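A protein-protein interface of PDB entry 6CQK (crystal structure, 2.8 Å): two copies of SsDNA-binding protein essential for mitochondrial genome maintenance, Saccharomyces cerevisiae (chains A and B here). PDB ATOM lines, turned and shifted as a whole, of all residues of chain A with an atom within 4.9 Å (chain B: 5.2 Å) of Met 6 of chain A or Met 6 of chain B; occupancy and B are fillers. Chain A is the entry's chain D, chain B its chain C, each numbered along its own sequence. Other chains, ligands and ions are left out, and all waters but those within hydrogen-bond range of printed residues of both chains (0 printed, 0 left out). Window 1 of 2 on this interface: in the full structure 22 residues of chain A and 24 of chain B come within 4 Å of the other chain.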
ATOM      1  N   SER A   4     -31.191  30.785  10.336  1.00  0.00           N
ATOM      2  CA  SER A   4     -29.802  30.792  10.703  1.00  0.00           C
ATOM      3  C   SER A   4     -29.204  29.412  10.517  1.00  0.00           C
ATOM      4  O   SER A   4     -29.376  28.578  11.356  1.00  0.00           O
ATOM      5  CB  SER A   4     -29.604  31.290  12.142  1.00  0.00           C
ATOM      6  OG  SER A   4     -30.243  30.492  13.070  1.00  0.00           O
ATOM      7  N   LYS A   5     -28.494  29.194   9.426  1.00  0.00           N
ATOM      8  CA  LYS A   5     -27.884  27.897   9.162  1.00  0.00           C
ATOM      9  C   LYS A   5     -26.390  28.008   9.229  1.00  0.00           C
ATOM     10  O   LYS A   5     -25.860  29.063   8.977  1.00  0.00           O
ATOM     11  CB  LYS A   5     -28.301  27.291   7.828  1.00  0.00           C
ATOM     12  CG  LYS A   5     -28.013  28.152   6.634  1.00  0.00           C
ATOM     13  CD  LYS A   5     -28.528  27.562   5.341  1.00  0.00           C
ATOM     14  CE  LYS A   5     -27.420  26.657   4.769  1.00  0.00           C
ATOM     15  NZ  LYS A   5     -27.880  25.672   3.743  1.00  0.00           N
ATOM     16  N   MET A   6     -25.743  26.892   9.577  1.00  0.00           N
ATOM     17  CA  MET A   6     -24.286  26.747   9.615  1.00  0.00           C
ATOM     18  C   MET A   6     -23.812  25.672   8.639  1.00  0.00           C
ATOM     19  O   MET A   6     -24.448  24.642   8.493  1.00  0.00           O
ATOM     20  CB  MET A   6     -23.852  26.284  10.980  1.00  0.00           C
ATOM     21  CG  MET A   6     -22.357  26.246  11.139  1.00  0.00           C
ATOM     22  SD  MET A   6     -21.837  27.102  12.638  1.00  0.00           S
ATOM     23  CE  MET A   6     -20.363  26.316  13.094  1.00  0.00           C
ATOM     24  N   SER A   7     -22.697  25.932   7.954  1.00  0.00           N
ATOM     25  CA  SER A   7     -22.033  24.928   7.114  1.00  0.00           C
ATOM     26  C   SER A   7     -20.690  24.729   7.724  1.00  0.00           C
ATOM     27  O   SER A   7     -20.023  25.684   8.030  1.00  0.00           O
ATOM     28  CB  SER A   7     -21.921  25.401   5.675  1.00  0.00           C
ATOM     29  OG  SER A   7     -23.169  25.964   5.271  1.00  0.00           O
ATOM     30  N   ILE A   8     -20.319  23.491   7.929  1.00  0.00           N
ATOM     31  CA  ILE A   8     -19.045  23.134   8.525  1.00  0.00           C
ATOM     32  C   ILE A   8     -18.315  22.106   7.649  1.00  0.00           C
ATOM     33  O   ILE A   8     -18.915  21.155   7.175  1.00  0.00           O
ATOM     34  CB  ILE A   8     -19.274  22.484   9.894  1.00  0.00           C
ATOM     35  CG1 ILE A   8     -19.933  23.495  10.836  1.00  0.00           C
ATOM     36  CG2 ILE A   8     -17.974  21.973  10.502  1.00  0.00           C
ATOM     37  CD1 ILE A   8     -20.831  22.835  11.858  1.00  0.00           C
ATOM     38  N   TYR A  45     -17.951  21.635  17.458  1.00  0.00           N
ATOM     39  CA  TYR A  45     -19.373  21.946  17.269  1.00  0.00           C
ATOM     40  C   TYR A  45     -20.151  20.652  17.533  1.00  0.00           C
ATOM     41  O   TYR A  45     -19.815  19.597  16.938  1.00  0.00           O
ATOM     42  CB  TYR A  45     -19.645  22.423  15.825  1.00  0.00           C
ATOM     43  CG  TYR A  45     -18.987  23.747  15.513  1.00  0.00           C
ATOM     44  CD1 TYR A  45     -19.433  24.900  16.111  1.00  0.00           C
ATOM     45  CD2 TYR A  45     -17.915  23.842  14.606  1.00  0.00           C
ATOM     46  CE1 TYR A  45     -18.847  26.124  15.840  1.00  0.00           C
ATOM     47  CE2 TYR A  45     -17.336  25.066  14.297  1.00  0.00           C
ATOM     48  CZ  TYR A  45     -17.798  26.217  14.913  1.00  0.00           C
ATOM     49  OH  TYR A  45     -17.250  27.466  14.612  1.00  0.00           O
ATOM     50  N   VAL A  70     -21.077  19.341   6.618  1.00  0.00           N
ATOM     51  CA  VAL A  70     -22.405  19.312   7.267  1.00  0.00           C
ATOM     52  C   VAL A  70     -23.084  20.663   7.103  1.00  0.00           C
ATOM     53  O   VAL A  70     -22.432  21.693   7.221  1.00  0.00           O
ATOM     54  CB  VAL A  70     -22.256  19.025   8.786  1.00  0.00           C
ATOM     55  CG1 VAL A  70     -23.580  19.217   9.508  1.00  0.00           C
ATOM     56  CG2 VAL A  70     -21.692  17.634   8.992  1.00  0.00           C
ATOM     57  N   GLU A  71     -24.381  20.645   6.869  1.00  0.00           N
ATOM     58  CA  GLU A  71     -25.175  21.804   7.003  1.00  0.00           C
ATOM     59  C   GLU A  71     -26.098  21.571   8.174  1.00  0.00           C
ATOM     60  O   GLU A  71     -26.742  20.557   8.211  1.00  0.00           O
ATOM     61  CB  GLU A  71     -25.999  22.035   5.749  1.00  0.00           C
ATOM     62  CG  GLU A  71     -25.165  22.378   4.538  1.00  0.00           C
ATOM     63  CD  GLU A  71     -26.014  22.310   3.250  1.00  0.00           C
ATOM     64  OE1 GLU A  71     -26.366  23.409   2.765  1.00  0.00           O
ATOM     65  OE2 GLU A  71     -26.371  21.196   2.753  1.00  0.00           O
ATOM     66  N   ALA A  72     -26.259  22.557   9.056  1.00  0.00           N
ATOM     67  CA  ALA A  72     -27.109  22.404  10.206  1.00  0.00           C
ATOM     68  C   ALA A  72     -27.884  23.653  10.501  1.00  0.00           C
ATOM     69  O   ALA A  72     -27.423  24.778  10.331  1.00  0.00           O
ATOM     70  CB  ALA A  72     -26.268  22.022  11.384  1.00  0.00           C
ATOM     71  N   ALA A  74     -29.195  26.314  12.928  1.00  0.00           N
ATOM     72  CA  ALA A  74     -28.662  26.839  14.182  1.00  0.00           C
ATOM     73  C   ALA A  74     -29.678  27.568  14.985  1.00  0.00           C
ATOM     74  O   ALA A  74     -30.485  28.326  14.430  1.00  0.00           O
ATOM     75  CB  ALA A  74     -27.518  27.768  13.902  1.00  0.00           C
ATOM     76  N   LEU A  92     -27.409  22.902  17.054  1.00  0.00           N
ATOM     77  CA  LEU A  92     -27.106  22.717  15.662  1.00  0.00           C
ATOM     78  C   LEU A  92     -27.721  21.425  15.278  1.00  0.00           C
ATOM     79  O   LEU A  92     -27.176  20.339  15.571  1.00  0.00           O
ATOM     80  CB  LEU A  92     -25.589  22.632  15.412  1.00  0.00           C
ATOM     81  CG  LEU A  92     -24.737  23.901  15.482  1.00  0.00           C
ATOM     82  CD1 LEU A  92     -23.279  23.515  15.389  1.00  0.00           C
ATOM     83  CD2 LEU A  92     -25.070  24.886  14.390  1.00  0.00           C
ATOM     84  N   SER B   4     -15.965  26.882   9.139  1.00  0.00           N
ATOM     85  CA  SER B   4     -17.238  26.878   9.809  1.00  0.00           C
ATOM     86  C   SER B   4     -17.895  28.216   9.603  1.00  0.00           C
ATOM     87  O   SER B   4     -17.546  29.137  10.270  1.00  0.00           O
ATOM     88  CB  SER B   4     -17.059  26.497  11.281  1.00  0.00           C
ATOM     89  OG  SER B   4     -16.276  27.391  11.960  1.00  0.00           O
ATOM     90  N   LYS B   5     -18.822  28.324   8.654  1.00  0.00           N
ATOM     91  CA  LYS B   5     -19.502  29.601   8.356  1.00  0.00           C
ATOM     92  C   LYS B   5     -20.972  29.522   8.643  1.00  0.00           C
ATOM     93  O   LYS B   5     -21.551  28.481   8.552  1.00  0.00           O
ATOM     94  CB  LYS B   5     -19.323  30.102   6.889  1.00  0.00           C
ATOM     95  CG  LYS B   5     -19.749  29.140   5.779  1.00  0.00           C
ATOM     96  CD  LYS B   5     -19.309  29.560   4.282  1.00  0.00           C
ATOM     97  CE  LYS B   5     -17.762  29.664   4.014  1.00  0.00           C
ATOM     98  NZ  LYS B   5     -17.320  29.576   2.577  1.00  0.00           N
ATOM     99  N   MET B   6     -21.545  30.666   8.990  1.00  0.00           N
ATOM    100  CA  MET B   6     -22.960  30.817   9.258  1.00  0.00           C
ATOM    101  C   MET B   6     -23.595  31.789   8.280  1.00  0.00           C
ATOM    102  O   MET B   6     -23.038  32.852   7.997  1.00  0.00           O
ATOM    103  CB  MET B   6     -23.135  31.401  10.654  1.00  0.00           C
ATOM    104  CG  MET B   6     -24.567  31.484  11.115  1.00  0.00           C
ATOM    105  SD  MET B   6     -24.889  30.822  12.757  1.00  0.00           S
ATOM    106  CE  MET B   6     -24.046  29.282  12.894  1.00  0.00           C
ATOM    107  N   SER B   7     -24.821  31.487   7.860  1.00  0.00           N
ATOM    108  CA  SER B   7     -25.650  32.467   7.162  1.00  0.00           C
ATOM    109  C   SER B   7     -26.868  32.744   8.010  1.00  0.00           C
ATOM    110  O   SER B   7     -27.489  31.827   8.508  1.00  0.00           O
ATOM    111  CB  SER B   7     -26.061  31.915   5.831  1.00  0.00           C
ATOM    112  OG  SER B   7     -24.953  31.310   5.220  1.00  0.00           O
ATOM    113  N   ILE B   8     -27.222  34.002   8.158  1.00  0.00           N
ATOM    114  CA  ILE B   8     -28.365  34.414   8.956  1.00  0.00           C
ATOM    115  C   ILE B   8     -29.276  35.388   8.188  1.00  0.00           C
ATOM    116  O   ILE B   8     -28.812  36.296   7.556  1.00  0.00           O
ATOM    117  CB  ILE B   8     -27.872  35.171  10.215  1.00  0.00           C
ATOM    118  CG1 ILE B   8     -27.039  34.240  11.097  1.00  0.00           C
ATOM    119  CG2 ILE B   8     -29.027  35.735  11.044  1.00  0.00           C
ATOM    120  CD1 ILE B   8     -25.954  34.975  11.867  1.00  0.00           C
ATOM    121  N   TYR B  45     -27.646  36.593  17.752  1.00  0.00           N
ATOM    122  CA  TYR B  45     -26.318  36.284  17.300  1.00  0.00           C
ATOM    123  C   TYR B  45     -25.535  37.613  17.337  1.00  0.00           C
ATOM    124  O   TYR B  45     -25.979  38.604  16.786  1.00  0.00           O
ATOM    125  CB  TYR B  45     -26.359  35.721  15.882  1.00  0.00           C
ATOM    126  CG  TYR B  45     -27.041  34.372  15.769  1.00  0.00           C
ATOM    127  CD1 TYR B  45     -26.458  33.251  16.275  1.00  0.00           C
ATOM    128  CD2 TYR B  45     -28.280  34.212  15.150  1.00  0.00           C
ATOM    129  CE1 TYR B  45     -27.071  31.999  16.177  1.00  0.00           C
ATOM    130  CE2 TYR B  45     -28.911  32.974  15.053  1.00  0.00           C
ATOM    131  CZ  TYR B  45     -28.289  31.860  15.573  1.00  0.00           C
ATOM    132  OH  TYR B  45     -28.885  30.594  15.527  1.00  0.00           O
ATOM    133  N   VAL B  70     -26.813  38.055   6.461  1.00  0.00           N
ATOM    134  CA  VAL B  70     -25.408  38.103   6.798  1.00  0.00           C
ATOM    135  C   VAL B  70     -24.769  36.737   6.622  1.00  0.00           C
ATOM    136  O   VAL B  70     -25.348  35.721   6.962  1.00  0.00           O
ATOM    137  CB  VAL B  70     -25.261  38.518   8.262  1.00  0.00           C
ATOM    138  CG1 VAL B  70     -23.803  38.367   8.750  1.00  0.00           C
ATOM    139  CG2 VAL B  70     -25.809  39.945   8.480  1.00  0.00           C
ATOM    140  N   GLU B  71     -23.554  36.718   6.140  1.00  0.00           N
ATOM    141  CA  GLU B  71     -22.713  35.539   6.208  1.00  0.00           C
ATOM    142  C   GLU B  71     -21.559  35.861   7.094  1.00  0.00           C
ATOM    143  O   GLU B  71     -20.966  36.931   6.950  1.00  0.00           O
ATOM    144  CB  GLU B  71     -22.178  35.220   4.828  1.00  0.00           C
ATOM    145  CG  GLU B  71     -23.233  34.800   3.834  1.00  0.00           C
ATOM    146  CD  GLU B  71     -22.653  34.712   2.418  1.00  0.00           C
ATOM    147  OE1 GLU B  71     -22.398  33.575   1.990  1.00  0.00           O
ATOM    148  OE2 GLU B  71     -22.395  35.772   1.741  1.00  0.00           O
ATOM    149  N   ALA B  72     -21.170  34.948   7.956  1.00  0.00           N
ATOM    150  CA  ALA B  72     -20.101  35.226   8.915  1.00  0.00           C
ATOM    151  C   ALA B  72     -19.249  33.996   9.214  1.00  0.00           C
ATOM    152  O   ALA B  72     -19.751  32.858   9.265  1.00  0.00           O
ATOM    153  CB  ALA B  72     -20.722  35.723  10.218  1.00  0.00           C
ATOM    154  N   ASP B  73     -17.960  34.203   9.408  1.00  0.00           N
ATOM    155  CA  ASP B  73     -17.087  33.088   9.850  1.00  0.00           C
ATOM    156  C   ASP B  73     -17.272  32.824  11.325  1.00  0.00           C
ATOM    157  O   ASP B  73     -17.379  33.750  12.100  1.00  0.00           O
ATOM    158  CB  ASP B  73     -15.640  33.360   9.524  1.00  0.00           C
ATOM    159  CG  ASP B  73     -15.351  33.139   8.067  1.00  0.00           C
ATOM    160  OD1 ASP B  73     -15.843  32.107   7.539  1.00  0.00           O
ATOM    161  OD2 ASP B  73     -14.670  33.989   7.420  1.00  0.00           O
ATOM    162  N   ALA B  74     -17.429  31.554  11.665  1.00  0.00           N
ATOM    163  CA  ALA B  74     -17.767  31.149  13.024  1.00  0.00           C
ATOM    164  C   ALA B  74     -16.611  30.473  13.721  1.00  0.00           C
ATOM    165  O   ALA B  74     -15.907  29.671  13.107  1.00  0.00           O
ATOM    166  CB  ALA B  74     -18.946  30.176  13.020  1.00  0.00           C
ATOM    167  N   LEU B  92     -18.563  35.305  15.643  1.00  0.00           N
ATOM    168  CA  LEU B  92     -19.131  35.353  14.315  1.00  0.00           C
ATOM    169  C   LEU B  92     -18.649  36.602  13.659  1.00  0.00           C
ATOM    170  O   LEU B  92     -19.081  37.715  14.013  1.00  0.00           O
ATOM    171  CB  LEU B  92     -20.644  35.436  14.349  1.00  0.00           C
ATOM    172  CG  LEU B  92     -21.412  34.179  14.677  1.00  0.00           C
ATOM    173  CD1 LEU B  92     -22.855  34.563  14.839  1.00  0.00           C
ATOM    174  CD2 LEU B  92     -21.309  33.106  13.619  1.00  0.00           C
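The side-chain hydroxyl (OG) of Ser 4 of chain B sits at hydrogen-bond distance from the side-chain hydroxyl (OH) of Tyr 45 of chain A.
N of Ser 7 of chain A lies within hydrogen-bond range of O of Lys 5 of chain B (2.9 Å).
N of Ser 7 of chain B is in hydrogen-bond range of O of Lys 5 of chain A, at 2.9 Å.
The side-chain hydroxyl of Tyr 45 of chain B sits at hydrogen-bond distance from the side-chain hydroxyl of Ser 4 of chain A.
OH of Tyr 45 of chain B lies within hydrogen-bond range of O of Ala 74 of chain A.
The side-chain hydroxyl (OH) of Tyr 45 of chain A sits at hydrogen-bond distance from the backbone carbonyl oxygen (O) of Ala 74 of chain B (3.0 Å).
The side-chain hydroxyl (OG) of Ser 4 of chain B is in hydrogen-bond range of the backbone carbonyl oxygen (O) of Ala 74 of chain B.
O of Met 6 of chain B is in hydrogen-bond range of N of Ala 72 of chain B.
The side-chain hydroxyl of Ser 4 of chain A is in hydrogen-bond range of the backbone carbonyl oxygen of Ala 74 of chain A.
The side-chain amino group (NZ) of Lys 5 of chain A lies within salt-bridge range of the side-chain carboxylate (OE1) of Glu 71 of chain A, at 2.9 Å.
The backbone carbonyl oxygen of Ala 72 of chain A lies within hydrogen-bond range of the backbone NH of Met 6 of chain A (2.8 Å).
Among the printed residues, merely in contact across the chains: Met 6 of chain A with Met 6 of chain B (3.1 Å), Ser 4 of chain A with Ser 7 of chain B (3.4 Å), Lys 5 of chain A with Met 6 of chain B (3.4 Å), Met 6 of chain A with Lys 5 of chain B (3.4 Å), Ser 7 of chain A with Ser 4 of chain B (3.5 Å), Met 6 of chain A with Ser 4 of chain B (3.8 Å) and Ala 74 of chain A with Met 6 of chain B (3.9 Å).
Printed residues of chain B within 4 Å of Ser 4 of chain A: Ser 7 and Tyr 45.
Of chain B, only Ser 4 (3.8 Å), Lys 5 (3.4 Å) and Met 6 (3.1 Å) come within 4 Å of Met 6 of chain A.
Of the printed residues of chain B, Tyr 45 of chain A touches Ser 4 and Ala 74.
Of the printed residues of chain B, Ala 74 of chain A touches Met 6 and Tyr 45.
Met 6 of chain B touches just these residues of chain A: Lys 5, Met 6 and Ala 74.
Val 70 of chain B touches none of the printed residues of chain A.
Printed residues of chain A within 4 Å of Ala 74 of chain B: Tyr 45.
The nearest residue of chain B that does not touch Met 6 of chain A is Ala 74 of chain B (4.1 Å).
The nearest printed residue of chain A that does not touch Met 6 of chain B is Leu 92 of chain A (4.8 Å).
The nearest printed residue of chain B that does not touch Ser 4 of chain A is Ile 8 of chain B (4.05 Å).
Of the 11 printed residues of chain A, 6 touch a printed residue of chain B.
Hydrophobic or aromatic side chains of chain A that line the printed part of chain B: Met 6, Tyr 45 and Ala 74.
Among the printed residues, 13 pairs touch across the chains.
Among the printed residues, no Asp or Glu carboxylate lies within 4 Å of a Lys or Arg side-chain nitrogen of the other chain.
Ser 4 of chain A touches Tyr 45 of chain B, and with the chains exchanged Tyr 45 of chain A touches Ser 4 of chain B.
Lys 5 of chain A touches Met 6 of chain B, and with the chains exchanged Met 6 of chain A touches Lys 5 of chain B.
Met 6 of chain B touches its own counterpart, Met 6 of chain A.
Ala 74 of chain A touches Met 6 of chain B, but with the chains exchanged Met 6 of chain A does not touch Ala 74 of chain B (4.1 Å).
Positions printed for both chains: 4, 5, 6, 7, 8, 45, 70, 71, 72, 74 and 92.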
